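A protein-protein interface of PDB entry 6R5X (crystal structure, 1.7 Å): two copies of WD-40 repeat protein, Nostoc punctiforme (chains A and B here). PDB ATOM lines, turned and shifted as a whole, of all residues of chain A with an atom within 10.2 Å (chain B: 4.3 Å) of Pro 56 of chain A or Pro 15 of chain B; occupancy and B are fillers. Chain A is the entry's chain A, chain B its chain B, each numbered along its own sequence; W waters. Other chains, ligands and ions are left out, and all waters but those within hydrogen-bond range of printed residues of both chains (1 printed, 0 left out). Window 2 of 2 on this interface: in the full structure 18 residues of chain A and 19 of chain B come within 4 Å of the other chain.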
ATOM      1  N   PHE A  13       1.049   3.705 -15.140  1.00  0.00           N
ATOM      2  CA  PHE A  13      -0.119   4.558 -15.454  1.00  0.00           C
ATOM      3  C   PHE A  13      -0.615   5.305 -14.240  1.00  0.00           C
ATOM      4  O   PHE A  13      -0.685   4.724 -13.137  1.00  0.00           O
ATOM      5  CB  PHE A  13      -1.193   3.625 -15.987  1.00  0.00           C
ATOM      6  CG  PHE A  13      -0.659   2.718 -17.062  1.00  0.00           C
ATOM      7  CD1 PHE A  13      -0.544   3.167 -18.371  1.00  0.00           C
ATOM      8  CD2 PHE A  13      -0.153   1.455 -16.750  1.00  0.00           C
ATOM      9  CE1 PHE A  13      -0.008   2.355 -19.373  1.00  0.00           C
ATOM     10  CE2 PHE A  13       0.382   0.639 -17.743  1.00  0.00           C
ATOM     11  CZ  PHE A  13       0.469   1.097 -19.056  1.00  0.00           C
ATOM     12  N   SER A  14      -0.961   6.578 -14.419  1.00  0.00           N
ATOM     13  CA  SER A  14      -1.521   7.343 -13.323  1.00  0.00           C
ATOM     14  C   SER A  14      -2.869   6.712 -12.889  1.00  0.00           C
ATOM     15  O   SER A  14      -3.542   6.036 -13.682  1.00  0.00           O
ATOM     16  CB  SER A  14      -1.735   8.817 -13.689  1.00  0.00           C
ATOM     17  OG  SER A  14      -2.662   8.971 -14.732  1.00  0.00           O
ATOM     18  N   PRO A  15      -3.259   6.932 -11.629  1.00  0.00           N
ATOM     19  CA  PRO A  15      -4.497   6.295 -11.162  1.00  0.00           C
ATOM     20  C   PRO A  15      -5.775   6.737 -11.926  1.00  0.00           C
ATOM     21  O   PRO A  15      -6.724   5.958 -11.982  1.00  0.00           O
ATOM     22  CB  PRO A  15      -4.564   6.655  -9.672  1.00  0.00           C
ATOM     23  CG  PRO A  15      -3.231   7.219  -9.311  1.00  0.00           C
ATOM     24  CD  PRO A  15      -2.453   7.522 -10.546  1.00  0.00           C
ATOM     25  N   ASP A  16      -5.788   7.937 -12.518  1.00  0.00           N
ATOM     26  CA  ASP A  16      -6.907   8.370 -13.363  1.00  0.00           C
ATOM     27  C   ASP A  16      -6.780   8.005 -14.849  1.00  0.00           C
ATOM     28  O   ASP A  16      -7.622   8.379 -15.680  1.00  0.00           O
ATOM     29  CB  ASP A  16      -7.175   9.875 -13.207  1.00  0.00           C
ATOM     30  CG  ASP A  16      -6.105  10.776 -13.836  1.00  0.00           C
ATOM     31  OD1 ASP A  16      -5.109  10.314 -14.460  1.00  0.00           O
ATOM     32  OD2 ASP A  16      -6.304  12.003 -13.694  1.00  0.00           O
ATOM     33  N   GLY A  17      -5.699   7.306 -15.186  1.00  0.00           N
ATOM     34  CA  GLY A  17      -5.504   6.798 -16.540  1.00  0.00           C
ATOM     35  C   GLY A  17      -5.127   7.840 -17.583  1.00  0.00           C
ATOM     36  O   GLY A  17      -5.050   7.504 -18.766  1.00  0.00           O
ATOM     37  N   ALA A  53       6.808   4.900 -10.805  1.00  0.00           N
ATOM     38  CA  ALA A  53       5.562   4.796 -10.027  1.00  0.00           C
ATOM     39  C   ALA A  53       4.947   6.173  -9.855  1.00  0.00           C
ATOM     40  O   ALA A  53       5.660   7.178  -9.848  1.00  0.00           O
ATOM     41  CB  ALA A  53       5.829   4.187  -8.648  1.00  0.00           C
ATOM     42  N   PHE A  54       3.609   6.216  -9.765  1.00  0.00           N
ATOM     43  CA  PHE A  54       2.873   7.442  -9.473  1.00  0.00           C
ATOM     44  C   PHE A  54       2.351   7.478  -8.040  1.00  0.00           C
ATOM     45  O   PHE A  54       1.952   6.435  -7.458  1.00  0.00           O
ATOM     46  CB  PHE A  54       1.658   7.565 -10.362  1.00  0.00           C
ATOM     47  CG  PHE A  54       1.959   7.907 -11.795  1.00  0.00           C
ATOM     48  CD1 PHE A  54       2.197   6.898 -12.723  1.00  0.00           C
ATOM     49  CD2 PHE A  54       1.985   9.228 -12.223  1.00  0.00           C
ATOM     50  CE1 PHE A  54       2.430   7.215 -14.044  1.00  0.00           C
ATOM     51  CE2 PHE A  54       2.201   9.551 -13.544  1.00  0.00           C
ATOM     52  CZ  PHE A  54       2.442   8.540 -14.461  1.00  0.00           C
ATOM     53  N   SER A  55       2.325   8.692  -7.479  1.00  0.00           N
ATOM     54  CA  SER A  55       1.667   8.950  -6.196  1.00  0.00           C
ATOM     55  C   SER A  55       0.117   8.825  -6.336  1.00  0.00           C
ATOM     56  O   SER A  55      -0.398   8.757  -7.441  1.00  0.00           O
ATOM     57  CB  SER A  55       2.019  10.343  -5.688  1.00  0.00           C
ATOM     58  OG  SER A  55       1.464  11.324  -6.538  1.00  0.00           O
ATOM     59  N   PRO A  56      -0.617   8.746  -5.216  1.00  0.00           N
ATOM     60  CA  PRO A  56      -2.086   8.504  -5.324  1.00  0.00           C
ATOM     61  C   PRO A  56      -2.926   9.508  -6.146  1.00  0.00           C
ATOM     62  O   PRO A  56      -3.962   9.127  -6.688  1.00  0.00           O
ATOM     63  CB  PRO A  56      -2.549   8.481  -3.859  1.00  0.00           C
ATOM     64  CG  PRO A  56      -1.329   8.023  -3.109  1.00  0.00           C
ATOM     65  CD  PRO A  56      -0.145   8.593  -3.821  1.00  0.00           C
ATOM     66  N   ASP A  57      -2.483  10.759  -6.217  1.00  0.00           N
ATOM     67  CA  ASP A  57      -3.150  11.783  -7.032  1.00  0.00           C
ATOM     68  C   ASP A  57      -2.498  11.990  -8.416  1.00  0.00           C
ATOM     69  O   ASP A  57      -2.932  12.853  -9.200  1.00  0.00           O
ATOM     70  CB  ASP A  57      -3.243  13.111  -6.253  1.00  0.00           C
ATOM     71  CG  ASP A  57      -1.892  13.769  -5.971  1.00  0.00           C
ATOM     72  OD1 ASP A  57      -0.815  13.288  -6.410  1.00  0.00           O
ATOM     73  OD2 ASP A  57      -1.954  14.835  -5.274  1.00  0.00           O
ATOM     74  N   GLY A  58      -1.447  11.228  -8.683  1.00  0.00           N
ATOM     75  CA  GLY A  58      -0.758  11.313  -9.964  1.00  0.00           C
ATOM     76  C   GLY A  58       0.190  12.495 -10.136  1.00  0.00           C
ATOM     77  O   GLY A  58       0.729  12.675 -11.225  1.00  0.00           O
ATOM     78  N   GLN A  59       0.338  13.346  -9.114  1.00  0.00           N
ATOM     79  CA  GLN A  59       1.117  14.580  -9.264  1.00  0.00           C
ATOM     80  C   GLN A  59       2.606  14.400  -9.026  1.00  0.00           C
ATOM     81  O   GLN A  59       3.367  15.285  -9.392  1.00  0.00           O
ATOM     82  CB  GLN A  59       0.596  15.654  -8.316  1.00  0.00           C
ATOM     83  CG  GLN A  59      -0.873  15.972  -8.518  1.00  0.00           C
ATOM     84  CD  GLN A  59      -1.221  16.284  -9.959  1.00  0.00           C
ATOM     85  OE1 GLN A  59      -0.826  17.326 -10.514  1.00  0.00           O
ATOM     86  NE2 GLN A  59      -1.998  15.401 -10.569  1.00  0.00           N
ATOM     87  N   THR A  60       2.988  13.324  -8.351  1.00  0.00           N
ATOM     88  CA  THR A  60       4.406  13.008  -8.137  1.00  0.00           C
ATOM     89  C   THR A  60       4.748  11.683  -8.783  1.00  0.00           C
ATOM     90  O   THR A  60       3.981  10.725  -8.681  1.00  0.00           O
ATOM     91  CB  THR A  60       4.773  12.983  -6.617  1.00  0.00           C
ATOM     92  OG1 THR A  60       4.330  14.195  -5.987  1.00  0.00           O
ATOM     93  CG2 THR A  60       6.292  12.838  -6.399  1.00  0.00           C
ATOM     94  N   ILE A  61       5.935  11.638  -9.383  1.00  0.00           N
ATOM     95  CA  ILE A  61       6.455  10.453 -10.038  1.00  0.00           C
ATOM     96  C   ILE A  61       7.714  10.056  -9.312  1.00  0.00           C
ATOM     97  O   ILE A  61       8.546  10.923  -9.052  1.00  0.00           O
ATOM     98  CB  ILE A  61       6.766  10.754 -11.534  1.00  0.00           C
ATOM     99  CG1 ILE A  61       5.481  11.106 -12.316  1.00  0.00           C
ATOM    100  CG2 ILE A  61       7.433   9.559 -12.196  1.00  0.00           C
ATOM    101  CD1 ILE A  61       5.105  12.571 -12.347  1.00  0.00           C
ATOM    102  N   ALA A  62       7.875   8.763  -9.037  1.00  0.00           N
ATOM    103  CA  ALA A  62       9.136   8.238  -8.541  1.00  0.00           C
ATOM    104  C   ALA A  62       9.838   7.376  -9.617  1.00  0.00           C
ATOM    105  O   ALA A  62       9.177   6.622 -10.364  1.00  0.00           O
ATOM    106  CB  ALA A  62       8.895   7.434  -7.309  1.00  0.00           C
ATOM    107  N   ARG A  75       4.796  16.295 -11.783  1.00  0.00           N
ATOM    108  CA  ARG A  75       4.376  15.993 -13.143  1.00  0.00           C
ATOM    109  C   ARG A  75       4.630  17.118 -14.130  1.00  0.00           C
ATOM    110  O   ARG A  75       4.591  16.893 -15.342  1.00  0.00           O
ATOM    111  CB  ARG A  75       2.912  15.510 -13.185  1.00  0.00           C
ATOM    112  CG  ARG A  75       1.859  16.584 -13.122  1.00  0.00           C
ATOM    113  CD  ARG A  75       0.492  15.895 -13.195  1.00  0.00           C
ATOM    114  NE  ARG A  75       0.230  15.181 -14.465  1.00  0.00           N
ATOM    115  CZ  ARG A  75      -0.046  15.753 -15.635  1.00  0.00           C
ATOM    116  NH1 ARG A  75      -0.101  17.080 -15.754  1.00  0.00           N
ATOM    117  NH2 ARG A  75      -0.259  14.986 -16.704  1.00  0.00           N
ATOM    118  N   PHE B  13       4.611   4.121  -3.794  1.00  0.00           N
ATOM    119  CA  PHE B  13       4.156   5.118  -2.811  1.00  0.00           C
ATOM    120  C   PHE B  13       3.137   4.474  -1.864  1.00  0.00           C
ATOM    121  O   PHE B  13       2.286   3.656  -2.268  1.00  0.00           O
ATOM    122  CB  PHE B  13       3.436   6.323  -3.462  1.00  0.00           C
ATOM    123  CG  PHE B  13       4.321   7.276  -4.219  1.00  0.00           C
ATOM    124  CD1 PHE B  13       4.643   7.048  -5.556  1.00  0.00           C
ATOM    125  CD2 PHE B  13       4.747   8.453  -3.622  1.00  0.00           C
ATOM    126  CE1 PHE B  13       5.431   7.950  -6.260  1.00  0.00           C
ATOM    127  CE2 PHE B  13       5.532   9.344  -4.322  1.00  0.00           C
ATOM    128  CZ  PHE B  13       5.883   9.083  -5.644  1.00  0.00           C
ATOM    129  N   SER B  14       3.214   4.832  -0.583  1.00  0.00           N
ATOM    130  CA  SER B  14       2.146   4.506   0.381  1.00  0.00           C
ATOM    131  C   SER B  14       0.790   5.120  -0.041  1.00  0.00           C
ATOM    132  O   SER B  14       0.763   6.087  -0.819  1.00  0.00           O
ATOM    133  CB  SER B  14       2.521   4.992   1.784  1.00  0.00           C
ATOM    134  OG  SER B  14       2.634   6.418   1.792  1.00  0.00           O
ATOM    135  N   PRO B  15      -0.338   4.587   0.460  1.00  0.00           N
ATOM    136  CA  PRO B  15      -1.646   5.114   0.044  1.00  0.00           C
ATOM    137  C   PRO B  15      -1.875   6.576   0.440  1.00  0.00           C
ATOM    138  O   PRO B  15      -2.707   7.238  -0.207  1.00  0.00           O
ATOM    139  CB  PRO B  15      -2.674   4.182   0.694  1.00  0.00           C
ATOM    140  CG  PRO B  15      -1.923   3.035   1.216  1.00  0.00           C
ATOM    141  CD  PRO B  15      -0.463   3.312   1.175  1.00  0.00           C
ATOM    142  N   ASP B  16      -1.159   7.085   1.448  1.00  0.00           N
ATOM    143  CA  ASP B  16      -1.250   8.549   1.766  1.00  0.00           C
ATOM    144  C   ASP B  16      -0.187   9.409   1.072  1.00  0.00           C
ATOM    145  O   ASP B  16      -0.114  10.613   1.309  1.00  0.00           O
ATOM    146  CB  ASP B  16      -1.250   8.789   3.278  1.00  0.00           C
ATOM    147  CG  ASP B  16       0.099   8.564   3.941  1.00  0.00           C
ATOM    148  OD1 ASP B  16       1.120   8.171   3.292  1.00  0.00           O
ATOM    149  OD2 ASP B  16       0.129   8.764   5.183  1.00  0.00           O
ATOM    150  N   GLY B  17       0.627   8.791   0.234  1.00  0.00           N
ATOM    151  CA  GLY B  17       1.665   9.481  -0.540  1.00  0.00           C
ATOM    152  C   GLY B  17       2.885   9.984   0.213  1.00  0.00           C
ATOM    153  O   GLY B  17       3.788  10.602  -0.390  1.00  0.00           O
ATOM    154  N   PHE B  54       2.379  -1.955  -0.514  1.00  0.00           N
ATOM    155  CA  PHE B  54       1.715  -1.537   0.721  1.00  0.00           C
ATOM    156  C   PHE B  54       0.319  -2.155   0.815  1.00  0.00           C
ATOM    157  O   PHE B  54      -0.403  -2.240  -0.201  1.00  0.00           O
ATOM    158  CB  PHE B  54       1.552  -0.014   0.778  1.00  0.00           C
ATOM    159  CG  PHE B  54       2.835   0.764   0.953  1.00  0.00           C
ATOM    160  CD1 PHE B  54       3.604   1.155  -0.157  1.00  0.00           C
ATOM    161  CD2 PHE B  54       3.277   1.108   2.217  1.00  0.00           C
ATOM    162  CE1 PHE B  54       4.787   1.864  -0.010  1.00  0.00           C
ATOM    163  CE2 PHE B  54       4.474   1.810   2.374  1.00  0.00           C
ATOM    164  CZ  PHE B  54       5.222   2.203   1.271  1.00  0.00           C
ATOM    165  N   SER B  55      -0.086  -2.468   2.038  1.00  0.00           N
ATOM    166  CA  SER B  55      -1.469  -2.823   2.310  1.00  0.00           C
ATOM    167  C   SER B  55      -2.396  -1.589   2.112  1.00  0.00           C
ATOM    168  O   SER B  55      -1.941  -0.457   2.051  1.00  0.00           O
ATOM    169  CB  SER B  55      -1.590  -3.366   3.715  1.00  0.00           C
ATOM    170  OG  SER B  55      -1.331  -2.361   4.673  1.00  0.00           O
ATOM    171  N   PRO B  56      -3.715  -1.807   1.985  1.00  0.00           N
ATOM    172  CA  PRO B  56      -4.638  -0.700   1.707  1.00  0.00           C
ATOM    173  C   PRO B  56      -4.673   0.436   2.750  1.00  0.00           C
ATOM    174  O   PRO B  56      -4.990   1.579   2.394  1.00  0.00           O
ATOM    175  CB  PRO B  56      -5.997  -1.398   1.669  1.00  0.00           C
ATOM    176  CG  PRO B  56      -5.696  -2.793   1.256  1.00  0.00           C
ATOM    177  CD  PRO B  56      -4.376  -3.124   1.864  1.00  0.00           C
ATOM    178  N   GLY B  58      -1.924   1.173   4.513  1.00  0.00           N
ATOM    179  CA  GLY B  58      -0.551   1.657   4.558  1.00  0.00           C
ATOM    180  C   GLY B  58       0.268   1.209   5.771  1.00  0.00           C
ATOM    181  O   GLY B  58       1.442   1.587   5.880  1.00  0.00           O
HETATM  182  O   HOH W   1       2.972   3.702  -6.147  1.00  0.00           O
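The backbone carbonyl oxygen (O) of Ala 53 of chain A is in hydrogen-bond range of the backbone NH (N) of Ala 62 of chain A, 2.8 Å away. The side-chain carboxylate of Asp 57 of chain A sits at hydrogen-bond distance from the side-chain hydroxyl of Ser 55 of chain A (3.0 Å). The side-chain hydroxyl (OG) of Ser 55 of chain A sits at hydrogen-bond distance from the backbone NH (N) of Gln 59 of chain A (3.5 Å). N of Ser 55 of chain A sits at hydrogen-bond distance from O of Thr 60 of chain A (2.9 Å). The side-chain hydroxyl (OG) of Ser 14 of chain B is in hydrogen-bond range of the side-chain carboxylate (OD1) of Asp 16 of chain B (2.8 Å). OG of Ser 14 of chain B sits at hydrogen-bond distance from N of Gly 17 of chain B, 3.5 Å away.
Among the printed residues, pairs that only touch across the chains: Pro 56 of chain A with Pro 15 of chain B (3.3 Å), Phe 54 of chain A with Phe 13 of chain B (3.4 Å), Ser 55 of chain A with Phe 13 of chain B (3.4 Å), Ala 62 of chain A with Phe 13 of chain B (3.7 Å), Pro 56 of chain A with Ser 14 of chain B (3.7 Å), Ala 53 of chain A with Phe 13 of chain B (3.7 Å), Pro 56 of chain A with Gly 17 of chain B (3.9 Å) and Thr 60 of chain A with Phe 13 of chain B (3.9 Å).
Pro 15 of chain B touches one residue of chain A. Of chain A, only Pro 56 comes within 4 Å of Ser 14 of chain B. Asp 16 of chain B touches none of the printed residues of chain A. Gly 17 of chain B touches one residue of chain A. No residue of chain A comes within 4 Å of Gly 58 of chain B. Printed residues of chain B within 4 Å of Ser 55 of chain A: Phe 13 (3.4 Å). Printed residues of chain B within 4 Å of Ala 53 of chain A: Phe 13. Phe 54 of chain B touches none of the printed residues of chain A. The nearest printed residue of chain B that does not touch Pro 56 of chain A is Phe 13 of chain B (4.3 Å). The nearest residue of chain A that does not touch Pro 15 of chain B is Ser 55 of chain A (6.9 Å).
Hydrophobic or aromatic side chains of chain B that line the printed part of chain A: Phe 13. Among the printed residues, no Asp or Glu carboxylate lies within 4 Å of a Lys or Arg side-chain nitrogen of the other chain.
Phe 54 of chain A touches Phe 13 of chain B, but with the chains exchanged Phe 13 of chain A does not touch Phe 54 of chain B (14.1 Å). Ser 55 of chain A touches Phe 13 of chain B, but with the chains exchanged Phe 13 of chain A does not touch Ser 55 of chain B (16.1 Å). Pro 56 of chain A touches Ser 14 of chain B, but with the chains exchanged Ser 14 of chain A does not touch Pro 56 of chain B (16.3 Å). Pro 56 of chain A touches Pro 15 of chain B, but with the chains exchanged Pro 15 of chain A does not touch Pro 56 of chain B (13.1 Å). Positions printed for both chains: 13, 14, 15, 16, 17, 54, 55, 56 and 58. Of the 8 pairs that touch across the chains among the printed residues, none has its exchanged pair printed and touching as well.
Water W1 bridges N of Phe 13 of chain B (2.9 Å) and O of Phe 54 of chain A (3.2 Å).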
